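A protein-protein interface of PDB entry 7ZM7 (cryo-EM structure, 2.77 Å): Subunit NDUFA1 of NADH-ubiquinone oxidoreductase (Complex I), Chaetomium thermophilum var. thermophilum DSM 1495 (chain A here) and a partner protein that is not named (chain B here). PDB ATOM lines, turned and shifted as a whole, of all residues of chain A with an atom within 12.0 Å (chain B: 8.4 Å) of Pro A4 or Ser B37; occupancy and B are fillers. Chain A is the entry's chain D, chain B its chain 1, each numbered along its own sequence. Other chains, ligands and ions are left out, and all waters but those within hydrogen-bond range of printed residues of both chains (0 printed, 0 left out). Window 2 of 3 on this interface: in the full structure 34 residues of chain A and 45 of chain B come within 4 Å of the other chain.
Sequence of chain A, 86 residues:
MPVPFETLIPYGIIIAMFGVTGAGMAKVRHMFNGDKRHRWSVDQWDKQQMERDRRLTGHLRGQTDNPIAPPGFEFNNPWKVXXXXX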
ATOM      1  N   PRO A   2      -0.745 -17.887  25.703  1.00  0.00           N
ATOM      2  CA  PRO A   2      -1.943 -17.451  24.990  1.00  0.00           C
ATOM      3  C   PRO A   2      -2.635 -18.609  24.296  1.00  0.00           C
ATOM      4  O   PRO A   2      -2.060 -19.676  24.143  1.00  0.00           O
ATOM      5  CB  PRO A   2      -1.406 -16.454  23.964  1.00  0.00           C
ATOM      6  CG  PRO A   2      -0.002 -16.225  24.319  1.00  0.00           C
ATOM      7  CD  PRO A   2       0.474 -17.424  25.037  1.00  0.00           C
ATOM      8  N   VAL A   3      -3.858 -18.376  23.849  1.00  0.00           N
ATOM      9  CA  VAL A   3      -4.706 -19.412  23.276  1.00  0.00           C
ATOM     10  C   VAL A   3      -4.650 -19.292  21.758  1.00  0.00           C
ATOM     11  O   VAL A   3      -4.989 -18.229  21.224  1.00  0.00           O
ATOM     12  CB  VAL A   3      -6.142 -19.289  23.786  1.00  0.00           C
ATOM     13  CG1 VAL A   3      -6.997 -20.355  23.170  1.00  0.00           C
ATOM     14  CG2 VAL A   3      -6.139 -19.372  25.279  1.00  0.00           C
ATOM     15  N   PRO A   4      -4.237 -20.313  21.047  1.00  0.00           N
ATOM     16  CA  PRO A   4      -4.119 -20.195  19.589  1.00  0.00           C
ATOM     17  C   PRO A   4      -5.420 -20.553  18.885  1.00  0.00           C
ATOM     18  O   PRO A   4      -5.586 -21.615  18.303  1.00  0.00           O
ATOM     19  CB  PRO A   4      -3.006 -21.190  19.270  1.00  0.00           C
ATOM     20  CG  PRO A   4      -3.193 -22.246  20.268  1.00  0.00           C
ATOM     21  CD  PRO A   4      -3.753 -21.619  21.519  1.00  0.00           C
ATOM     22  N   PHE A   5      -6.369 -19.629  18.915  1.00  0.00           N
ATOM     23  CA  PHE A   5      -7.708 -19.934  18.433  1.00  0.00           C
ATOM     24  C   PHE A   5      -7.741 -20.326  16.962  1.00  0.00           C
ATOM     25  O   PHE A   5      -8.696 -20.970  16.529  1.00  0.00           O
ATOM     26  CB  PHE A   5      -8.625 -18.741  18.677  1.00  0.00           C
ATOM     27  CG  PHE A   5      -8.298 -17.551  17.845  1.00  0.00           C
ATOM     28  CD1 PHE A   5      -7.310 -16.679  18.232  1.00  0.00           C
ATOM     29  CD2 PHE A   5      -8.983 -17.303  16.669  1.00  0.00           C
ATOM     30  CE1 PHE A   5      -7.019 -15.586  17.473  1.00  0.00           C
ATOM     31  CE2 PHE A   5      -8.683 -16.213  15.902  1.00  0.00           C
ATOM     32  CZ  PHE A   5      -7.704 -15.347  16.313  1.00  0.00           C
ATOM     33  N   GLU A   6      -6.726 -19.968  16.186  1.00  0.00           N
ATOM     34  CA  GLU A   6      -6.705 -20.371  14.786  1.00  0.00           C
ATOM     35  C   GLU A   6      -6.645 -21.883  14.650  1.00  0.00           C
ATOM     36  O   GLU A   6      -7.361 -22.464  13.829  1.00  0.00           O
ATOM     37  CB  GLU A   6      -5.514 -19.747  14.079  1.00  0.00           C
ATOM     38  CG  GLU A   6      -5.692 -18.301  13.760  1.00  0.00           C
ATOM     39  CD  GLU A   6      -5.103 -17.401  14.829  1.00  0.00           C
ATOM     40  OE1 GLU A   6      -5.357 -16.186  14.785  1.00  0.00           O
ATOM     41  OE2 GLU A   6      -4.397 -17.916  15.721  1.00  0.00           O
ATOM     42  N   THR A   7      -5.798 -22.539  15.441  1.00  0.00           N
ATOM     43  CA  THR A   7      -5.755 -23.990  15.408  1.00  0.00           C
ATOM     44  C   THR A   7      -7.060 -24.593  15.886  1.00  0.00           C
ATOM     45  O   THR A   7      -7.420 -25.693  15.461  1.00  0.00           O
ATOM     46  CB  THR A   7      -4.599 -24.525  16.257  1.00  0.00           C
ATOM     47  OG1 THR A   7      -4.839 -24.254  17.637  1.00  0.00           O
ATOM     48  CG2 THR A   7      -3.311 -23.856  15.859  1.00  0.00           C
ATOM     49  N   LEU A   8      -7.778 -23.883  16.744  1.00  0.00           N
ATOM     50  CA  LEU A   8      -9.068 -24.301  17.258  1.00  0.00           C
ATOM     51  C   LEU A   8     -10.207 -24.097  16.273  1.00  0.00           C
ATOM     52  O   LEU A   8     -11.271 -24.684  16.468  1.00  0.00           O
ATOM     53  CB  LEU A   8      -9.366 -23.541  18.547  1.00  0.00           C
ATOM     54  CG  LEU A   8      -8.695 -23.965  19.841  1.00  0.00           C
ATOM     55  CD1 LEU A   8      -7.245 -23.635  19.841  1.00  0.00           C
ATOM     56  CD2 LEU A   8      -9.366 -23.207  20.954  1.00  0.00           C
ATOM     57  N   ILE A   9     -10.014 -23.284  15.235  1.00  0.00           N
ATOM     58  CA  ILE A   9     -11.082 -23.054  14.257  1.00  0.00           C
ATOM     59  C   ILE A   9     -11.535 -24.337  13.570  1.00  0.00           C
ATOM     60  O   ILE A   9     -12.749 -24.574  13.499  1.00  0.00           O
ATOM     61  CB  ILE A   9     -10.656 -21.971  13.251  1.00  0.00           C
ATOM     62  CG1 ILE A   9     -10.917 -20.582  13.809  1.00  0.00           C
ATOM     63  CG2 ILE A   9     -11.385 -22.144  11.947  1.00  0.00           C
ATOM     64  CD1 ILE A   9     -10.347 -19.503  12.971  1.00  0.00           C
ATOM     65  N   PRO A  10     -10.647 -25.191  13.044  1.00  0.00           N
ATOM     66  CA  PRO A  10     -11.135 -26.438  12.431  1.00  0.00           C
ATOM     67  C   PRO A  10     -11.947 -27.321  13.352  1.00  0.00           C
ATOM     68  O   PRO A  10     -12.892 -27.955  12.885  1.00  0.00           O
ATOM     69  CB  PRO A  10      -9.841 -27.129  11.995  1.00  0.00           C
ATOM     70  CG  PRO A  10      -8.933 -26.034  11.757  1.00  0.00           C
ATOM     71  CD  PRO A  10      -9.205 -25.027  12.801  1.00  0.00           C
ATOM     72  N   TYR A  11     -11.590 -27.414  14.635  1.00  0.00           N
ATOM     73  CA  TYR A  11     -12.356 -28.258  15.548  1.00  0.00           C
ATOM     74  C   TYR A  11     -13.780 -27.747  15.686  1.00  0.00           C
ATOM     75  O   TYR A  11     -14.730 -28.535  15.703  1.00  0.00           O
ATOM     76  CB  TYR A  11     -11.677 -28.330  16.915  1.00  0.00           C
ATOM     77  CG  TYR A  11     -10.384 -29.092  16.908  1.00  0.00           C
ATOM     78  CD1 TYR A  11     -10.369 -30.465  17.065  1.00  0.00           C
ATOM     79  CD2 TYR A  11      -9.174 -28.443  16.744  1.00  0.00           C
ATOM     80  CE1 TYR A  11      -9.184 -31.169  17.060  1.00  0.00           C
ATOM     81  CE2 TYR A  11      -7.986 -29.140  16.736  1.00  0.00           C
ATOM     82  CZ  TYR A  11      -8.003 -30.496  16.890  1.00  0.00           C
ATOM     83  OH  TYR A  11      -6.827 -31.189  16.886  1.00  0.00           O
ATOM     84  N   GLY A  12     -13.946 -26.430  15.782  1.00  0.00           N
ATOM     85  CA  GLY A  12     -15.276 -25.864  15.808  1.00  0.00           C
ATOM     86  C   GLY A  12     -16.063 -26.149  14.551  1.00  0.00           C
ATOM     87  O   GLY A  12     -17.287 -26.243  14.594  1.00  0.00           O
ATOM     88  N   ILE A  13     -15.381 -26.279  13.416  1.00  0.00           N
ATOM     89  CA  ILE A  13     -16.065 -26.634  12.179  1.00  0.00           C
ATOM     90  C   ILE A  13     -16.650 -28.029  12.289  1.00  0.00           C
ATOM     91  O   ILE A  13     -17.807 -28.266  11.923  1.00  0.00           O
ATOM     92  CB  ILE A  13     -15.112 -26.522  10.981  1.00  0.00           C
ATOM     93  CG1 ILE A  13     -14.807 -25.060  10.662  1.00  0.00           C
ATOM     94  CG2 ILE A  13     -15.686 -27.232   9.783  1.00  0.00           C
ATOM     95  CD1 ILE A  13     -13.648 -24.907   9.746  1.00  0.00           C
ATOM     96  N   GLY B  30      -6.655 -29.687  10.700  1.00  0.00           N
ATOM     97  CA  GLY B  30      -6.559 -29.605  12.170  1.00  0.00           C
ATOM     98  C   GLY B  30      -5.337 -30.291  12.739  1.00  0.00           C
ATOM     99  O   GLY B  30      -4.758 -29.752  13.672  1.00  0.00           O
ATOM    100  N   GLU B  31      -4.898 -31.385  12.111  1.00  0.00           N
ATOM    101  CA  GLU B  31      -3.758 -32.186  12.627  1.00  0.00           C
ATOM    102  C   GLU B  31      -2.444 -31.462  12.333  1.00  0.00           C
ATOM    103  O   GLU B  31      -1.451 -31.730  13.033  1.00  0.00           O
ATOM    104  CB  GLU B  31      -3.741 -33.542  11.922  1.00  0.00           C
ATOM    105  CG  GLU B  31      -2.765 -34.539  12.516  1.00  0.00           C
ATOM    106  CD  GLU B  31      -2.011 -35.358  11.487  1.00  0.00           C
ATOM    107  OE1 GLU B  31      -1.746 -36.541  11.760  1.00  0.00           O
ATOM    108  OE2 GLU B  31      -1.684 -34.805  10.420  1.00  0.00           O
ATOM    109  N   ARG B  32      -2.462 -30.530  11.381  1.00  0.00           N
ATOM    110  CA  ARG B  32      -1.225 -29.810  11.005  1.00  0.00           C
ATOM    111  C   ARG B  32      -1.211 -28.537  11.843  1.00  0.00           C
ATOM    112  O   ARG B  32      -0.115 -28.103  12.239  1.00  0.00           O
ATOM    113  CB  ARG B  32      -1.224 -29.546   9.497  1.00  0.00           C
ATOM    114  CG  ARG B  32      -1.298 -30.798   8.640  1.00  0.00           C
ATOM    115  CD  ARG B  32      -1.652 -30.495   7.198  1.00  0.00           C
ATOM    116  NE  ARG B  32      -0.721 -29.592   6.541  1.00  0.00           N
ATOM    117  CZ  ARG B  32      -0.738 -29.317   5.242  1.00  0.00           C
ATOM    118  NH1 ARG B  32      -1.631 -29.891   4.455  1.00  0.00           N
ATOM    119  NH2 ARG B  32       0.146 -28.479   4.729  1.00  0.00           N
ATOM    120  N   LYS B  33      -2.395 -27.994  12.127  1.00  0.00           N
ATOM    121  CA  LYS B  33      -2.490 -26.800  13.008  1.00  0.00           C
ATOM    122  C   LYS B  33      -2.214 -27.148  14.479  1.00  0.00           C
ATOM    123  O   LYS B  33      -1.470 -26.398  15.115  1.00  0.00           O
ATOM    124  CB  LYS B  33      -3.775 -26.012  12.721  1.00  0.00           C
ATOM    125  CG  LYS B  33      -3.847 -25.380  11.340  1.00  0.00           C
ATOM    126  CD  LYS B  33      -4.745 -24.172  11.270  1.00  0.00           C
ATOM    127  CE  LYS B  33      -4.196 -22.972  12.013  1.00  0.00           C
ATOM    128  NZ  LYS B  33      -2.981 -22.415  11.375  1.00  0.00           N
ATOM    129  N   THR B  34      -2.764 -28.249  14.986  1.00  0.00           N
ATOM    130  CA  THR B  34      -2.538 -28.673  16.393  1.00  0.00           C
ATOM    131  C   THR B  34      -1.070 -29.035  16.635  1.00  0.00           C
ATOM    132  O   THR B  34      -0.518 -28.569  17.631  1.00  0.00           O
ATOM    133  CB  THR B  34      -3.426 -29.872  16.720  1.00  0.00           C
ATOM    134  OG1 THR B  34      -4.736 -29.547  16.265  1.00  0.00           O
ATOM    135  CG2 THR B  34      -3.476 -30.186  18.198  1.00  0.00           C
ATOM    136  N   MET B  35      -0.457 -29.786  15.719  1.00  0.00           N
ATOM    137  CA  MET B  35       0.948 -30.240  15.870  1.00  0.00           C
ATOM    138  C   MET B  35       1.872 -29.026  15.806  1.00  0.00           C
ATOM    139  O   MET B  35       2.920 -29.076  16.431  1.00  0.00           O
ATOM    140  CB  MET B  35       1.315 -31.278  14.806  1.00  0.00           C
ATOM    141  CG  MET B  35       2.002 -32.499  15.381  1.00  0.00           C
ATOM    142  SD  MET B  35       1.937 -33.949  14.302  1.00  0.00           S
ATOM    143  CE  MET B  35       0.358 -34.648  14.772  1.00  0.00           C
ATOM    144  N   GLY B  36       1.437 -27.946  15.164  1.00  0.00           N
ATOM    145  CA  GLY B  36       2.232 -26.712  15.083  1.00  0.00           C
ATOM    146  C   GLY B  36       2.133 -25.930  16.380  1.00  0.00           C
ATOM    147  O   GLY B  36       3.179 -25.429  16.802  1.00  0.00           O
ATOM    148  N   SER B  37       0.974 -25.855  17.041  1.00  0.00           N
ATOM    149  CA  SER B  37       0.965 -25.200  18.348  1.00  0.00           C
ATOM    150  C   SER B  37       1.793 -25.959  19.369  1.00  0.00           C
ATOM    151  O   SER B  37       2.469 -25.348  20.195  1.00  0.00           O
ATOM    152  CB  SER B  37      -0.457 -25.015  18.868  1.00  0.00           C
ATOM    153  OG  SER B  37      -1.163 -24.113  18.067  1.00  0.00           O
ATOM    154  N   MET B  38       1.725 -27.286  19.361  1.00  0.00           N
ATOM    155  CA  MET B  38       2.559 -28.036  20.289  1.00  0.00           C
ATOM    156  C   MET B  38       4.023 -27.996  19.892  1.00  0.00           C
ATOM    157  O   MET B  38       4.892 -28.174  20.746  1.00  0.00           O
ATOM    158  CB  MET B  38       2.061 -29.475  20.430  1.00  0.00           C
ATOM    159  CG  MET B  38       0.704 -29.541  21.101  1.00  0.00           C
ATOM    160  SD  MET B  38       0.004 -31.159  21.408  1.00  0.00           S
ATOM    161  CE  MET B  38      -0.474 -31.606  19.760  1.00  0.00           C
ATOM    162  N   GLN B  39       4.311 -27.739  18.610  1.00  0.00           N
ATOM    163  CA  GLN B  39       5.719 -27.626  18.145  1.00  0.00           C
ATOM    164  C   GLN B  39       6.115 -26.159  17.993  1.00  0.00           C
ATOM    165  O   GLN B  39       7.116 -25.913  17.302  1.00  0.00           O
ATOM    166  CB  GLN B  39       5.922 -28.404  16.848  1.00  0.00           C
ATOM    167  CG  GLN B  39       5.926 -29.914  17.034  1.00  0.00           C
ATOM    168  CD  GLN B  39       5.640 -30.679  15.764  1.00  0.00           C
ATOM    169  OE1 GLN B  39       5.355 -30.103  14.718  1.00  0.00           O
ATOM    170  NE2 GLN B  39       5.704 -31.996  15.852  1.00  0.00           N
ATOM    171  N   ARG B  40       5.358 -25.235  18.598  1.00  0.00           N
ATOM    172  CA  ARG B  40       5.694 -23.815  18.666  1.00  0.00           C
ATOM    173  C   ARG B  40       5.814 -23.184  17.294  1.00  0.00           C
ATOM    174  O   ARG B  40       6.578 -22.244  17.106  1.00  0.00           O
ATOM    175  CB  ARG B  40       6.972 -23.560  19.462  1.00  0.00           C
ATOM    176  CG  ARG B  40       6.997 -24.139  20.848  1.00  0.00           C
ATOM    177  CD  ARG B  40       6.250 -23.309  21.837  1.00  0.00           C
ATOM    178  NE  ARG B  40       6.662 -21.916  21.892  1.00  0.00           N
ATOM    179  CZ  ARG B  40       7.549 -21.421  22.741  1.00  0.00           C
ATOM    180  NH1 ARG B  40       8.165 -22.202  23.605  1.00  0.00           N
ATOM    181  NH2 ARG B  40       7.841 -20.138  22.706  1.00  0.00           N
ATOM    182  N   ARG B  41       5.023 -23.688  16.369  1.00  0.00           N
ATOM    183  CA  ARG B  41       4.998 -23.081  15.026  1.00  0.00           C
ATOM    184  C   ARG B  41       3.537 -22.850  14.681  1.00  0.00           C
ATOM    185  O   ARG B  41       2.708 -22.826  15.603  1.00  0.00           O
ATOM    186  CB  ARG B  41       5.684 -23.987  14.004  1.00  0.00           C
ATOM    187  CG  ARG B  41       5.262 -25.448  14.040  1.00  0.00           C
ATOM    188  CD  ARG B  41       5.781 -26.194  12.827  1.00  0.00           C
ATOM    189  NE  ARG B  41       5.258 -27.550  12.723  1.00  0.00           N
ATOM    190  CZ  ARG B  41       4.186 -27.889  12.020  1.00  0.00           C
ATOM    191  NH1 ARG B  41       3.515 -26.965  11.356  1.00  0.00           N
ATOM    192  NH2 ARG B  41       3.784 -29.147  11.985  1.00  0.00           N
ATOM    193  N   LEU B  42       3.254 -22.614  13.416  1.00  0.00           N
ATOM    194  CA  LEU B  42       1.890 -22.474  12.946  1.00  0.00           C
ATOM    195  C   LEU B  42       1.541 -23.646  12.041  1.00  0.00           C
ATOM    196  O   LEU B  42       2.414 -24.242  11.406  1.00  0.00           O
ATOM    197  CB  LEU B  42       1.731 -21.156  12.205  1.00  0.00           C
ATOM    198  CG  LEU B  42       2.012 -19.983  13.123  1.00  0.00           C
ATOM    199  CD1 LEU B  42       1.967 -18.690  12.357  1.00  0.00           C
ATOM    200  CD2 LEU B  42       0.999 -19.981  14.233  1.00  0.00           C
ATOM    201  N   GLY B  43       0.274 -23.991  11.995  1.00  0.00           N
ATOM    202  CA  GLY B  43      -0.181 -24.874  10.954  1.00  0.00           C
ATOM    203  C   GLY B  43      -0.372 -24.102   9.668  1.00  0.00           C
ATOM    204  O   GLY B  43       0.093 -22.974   9.527  1.00  0.00           O
ATOM    205  N   PHE B 325      -8.344 -34.759  19.139  1.00  0.00           N
ATOM    206  CA  PHE B 325      -7.202 -34.103  19.750  1.00  0.00           C
ATOM    207  C   PHE B 325      -6.249 -35.115  20.367  1.00  0.00           C
ATOM    208  O   PHE B 325      -5.029 -34.998  20.217  1.00  0.00           O
ATOM    209  CB  PHE B 325      -7.689 -33.108  20.802  1.00  0.00           C
ATOM    210  CG  PHE B 325      -6.637 -32.153  21.280  1.00  0.00           C
ATOM    211  CD1 PHE B 325      -5.760 -32.509  22.280  1.00  0.00           C
ATOM    212  CD2 PHE B 325      -6.538 -30.895  20.730  1.00  0.00           C
ATOM    213  CE1 PHE B 325      -4.803 -31.648  22.717  1.00  0.00           C
ATOM    214  CE2 PHE B 325      -5.578 -30.019  21.166  1.00  0.00           C
ATOM    215  CZ  PHE B 325      -4.706 -30.401  22.164  1.00  0.00           C
ATOM    216  N   ALA B 332       2.226 -36.585  18.379  1.00  0.00           N
ATOM    217  CA  ALA B 332       3.250 -35.558  18.650  1.00  0.00           C
ATOM    218  C   ALA B 332       4.005 -35.820  19.960  1.00  0.00           C
ATOM    219  O   ALA B 332       4.962 -35.100  20.221  1.00  0.00           O
ATOM    220  CB  ALA B 332       2.563 -34.220  18.649  1.00  0.00           C
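Among the printed residues, pairs that only touch across the chains: Pro A4 with Ser B37 (3.5 Å), Glu A6 with Lys B33 (3.7 Å), Thr A7 with Lys B33 (3.2 Å), Thr A7 with Ser B37 (3.1 Å) and Tyr A11 with Phe B325 (3.9 Å).
Of chain B, only Ser B37 (3.5 Å) comes within 4 Å of Pro A4.
Of chain A, only Pro A4 and Thr A7 come within 4 Å of Ser B37.
Printed residues of chain A within 4 Å of Lys B33: Glu A6 (3.7 Å) and Thr A7 (3.2 Å).
Of chain A, only Tyr A11 (2.7 Å) comes within 4 Å of Thr B34.
No residue of chain A comes within 4 Å of Gly B36.
No residue of chain A comes within 4 Å of Gln B39.
No residue of chain A comes within 4 Å of Arg B40.
Of the printed residues of chain A, Phe B325 touches Tyr A11 (3.9 Å).
Printed residues of chain B within 4 Å of Tyr A11: Thr B34 (2.7 Å) and Phe B325 (3.9 Å).
Of the printed residues of chain B, Glu A6 touches Lys B33 (3.7 Å).
Of the printed residues of chain B, Thr A7 touches Lys B33 and Ser B37.
Ile A13 touches none of the printed residues of chain B.
Gly B43 touches none of the printed residues of chain A.
The nearest residue of chain B that does not touch Pro A4 is Leu B42 (6.5 Å).
The nearest residue of chain A that does not touch Ser B37 is Leu A8 (6.4 Å).
The side-chain hydroxyl of Thr B34 sits at hydrogen-bond distance from the side-chain hydroxyl of Tyr A11.
The backbone carbonyl oxygen (O) of Gly B30 sits at hydrogen-bond distance from the side-chain hydroxyl (OG1) of Thr B34, at 2.6 Å.
O of Pro A4 is in hydrogen-bond range of OG1 of Thr A7 (2.8 Å).
Of the 16 printed residues of chain B, 4 touch a printed residue of chain A.
Hydrophobic or aromatic side chains of chain B within 4 Å of the printed part of chain A: Phe B325.
Of the 12 printed residues of chain A, 4 touch a printed residue of chain B.
Printed residues of chain A that touch a printed residue of chain B: Pro A4, Glu A6, Thr A7 and Tyr A11.
Along chain A the printed residues that touch a printed residue of chain B span positions 4 to 11.
Among the printed residues, 6 pairs touch across the chains.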
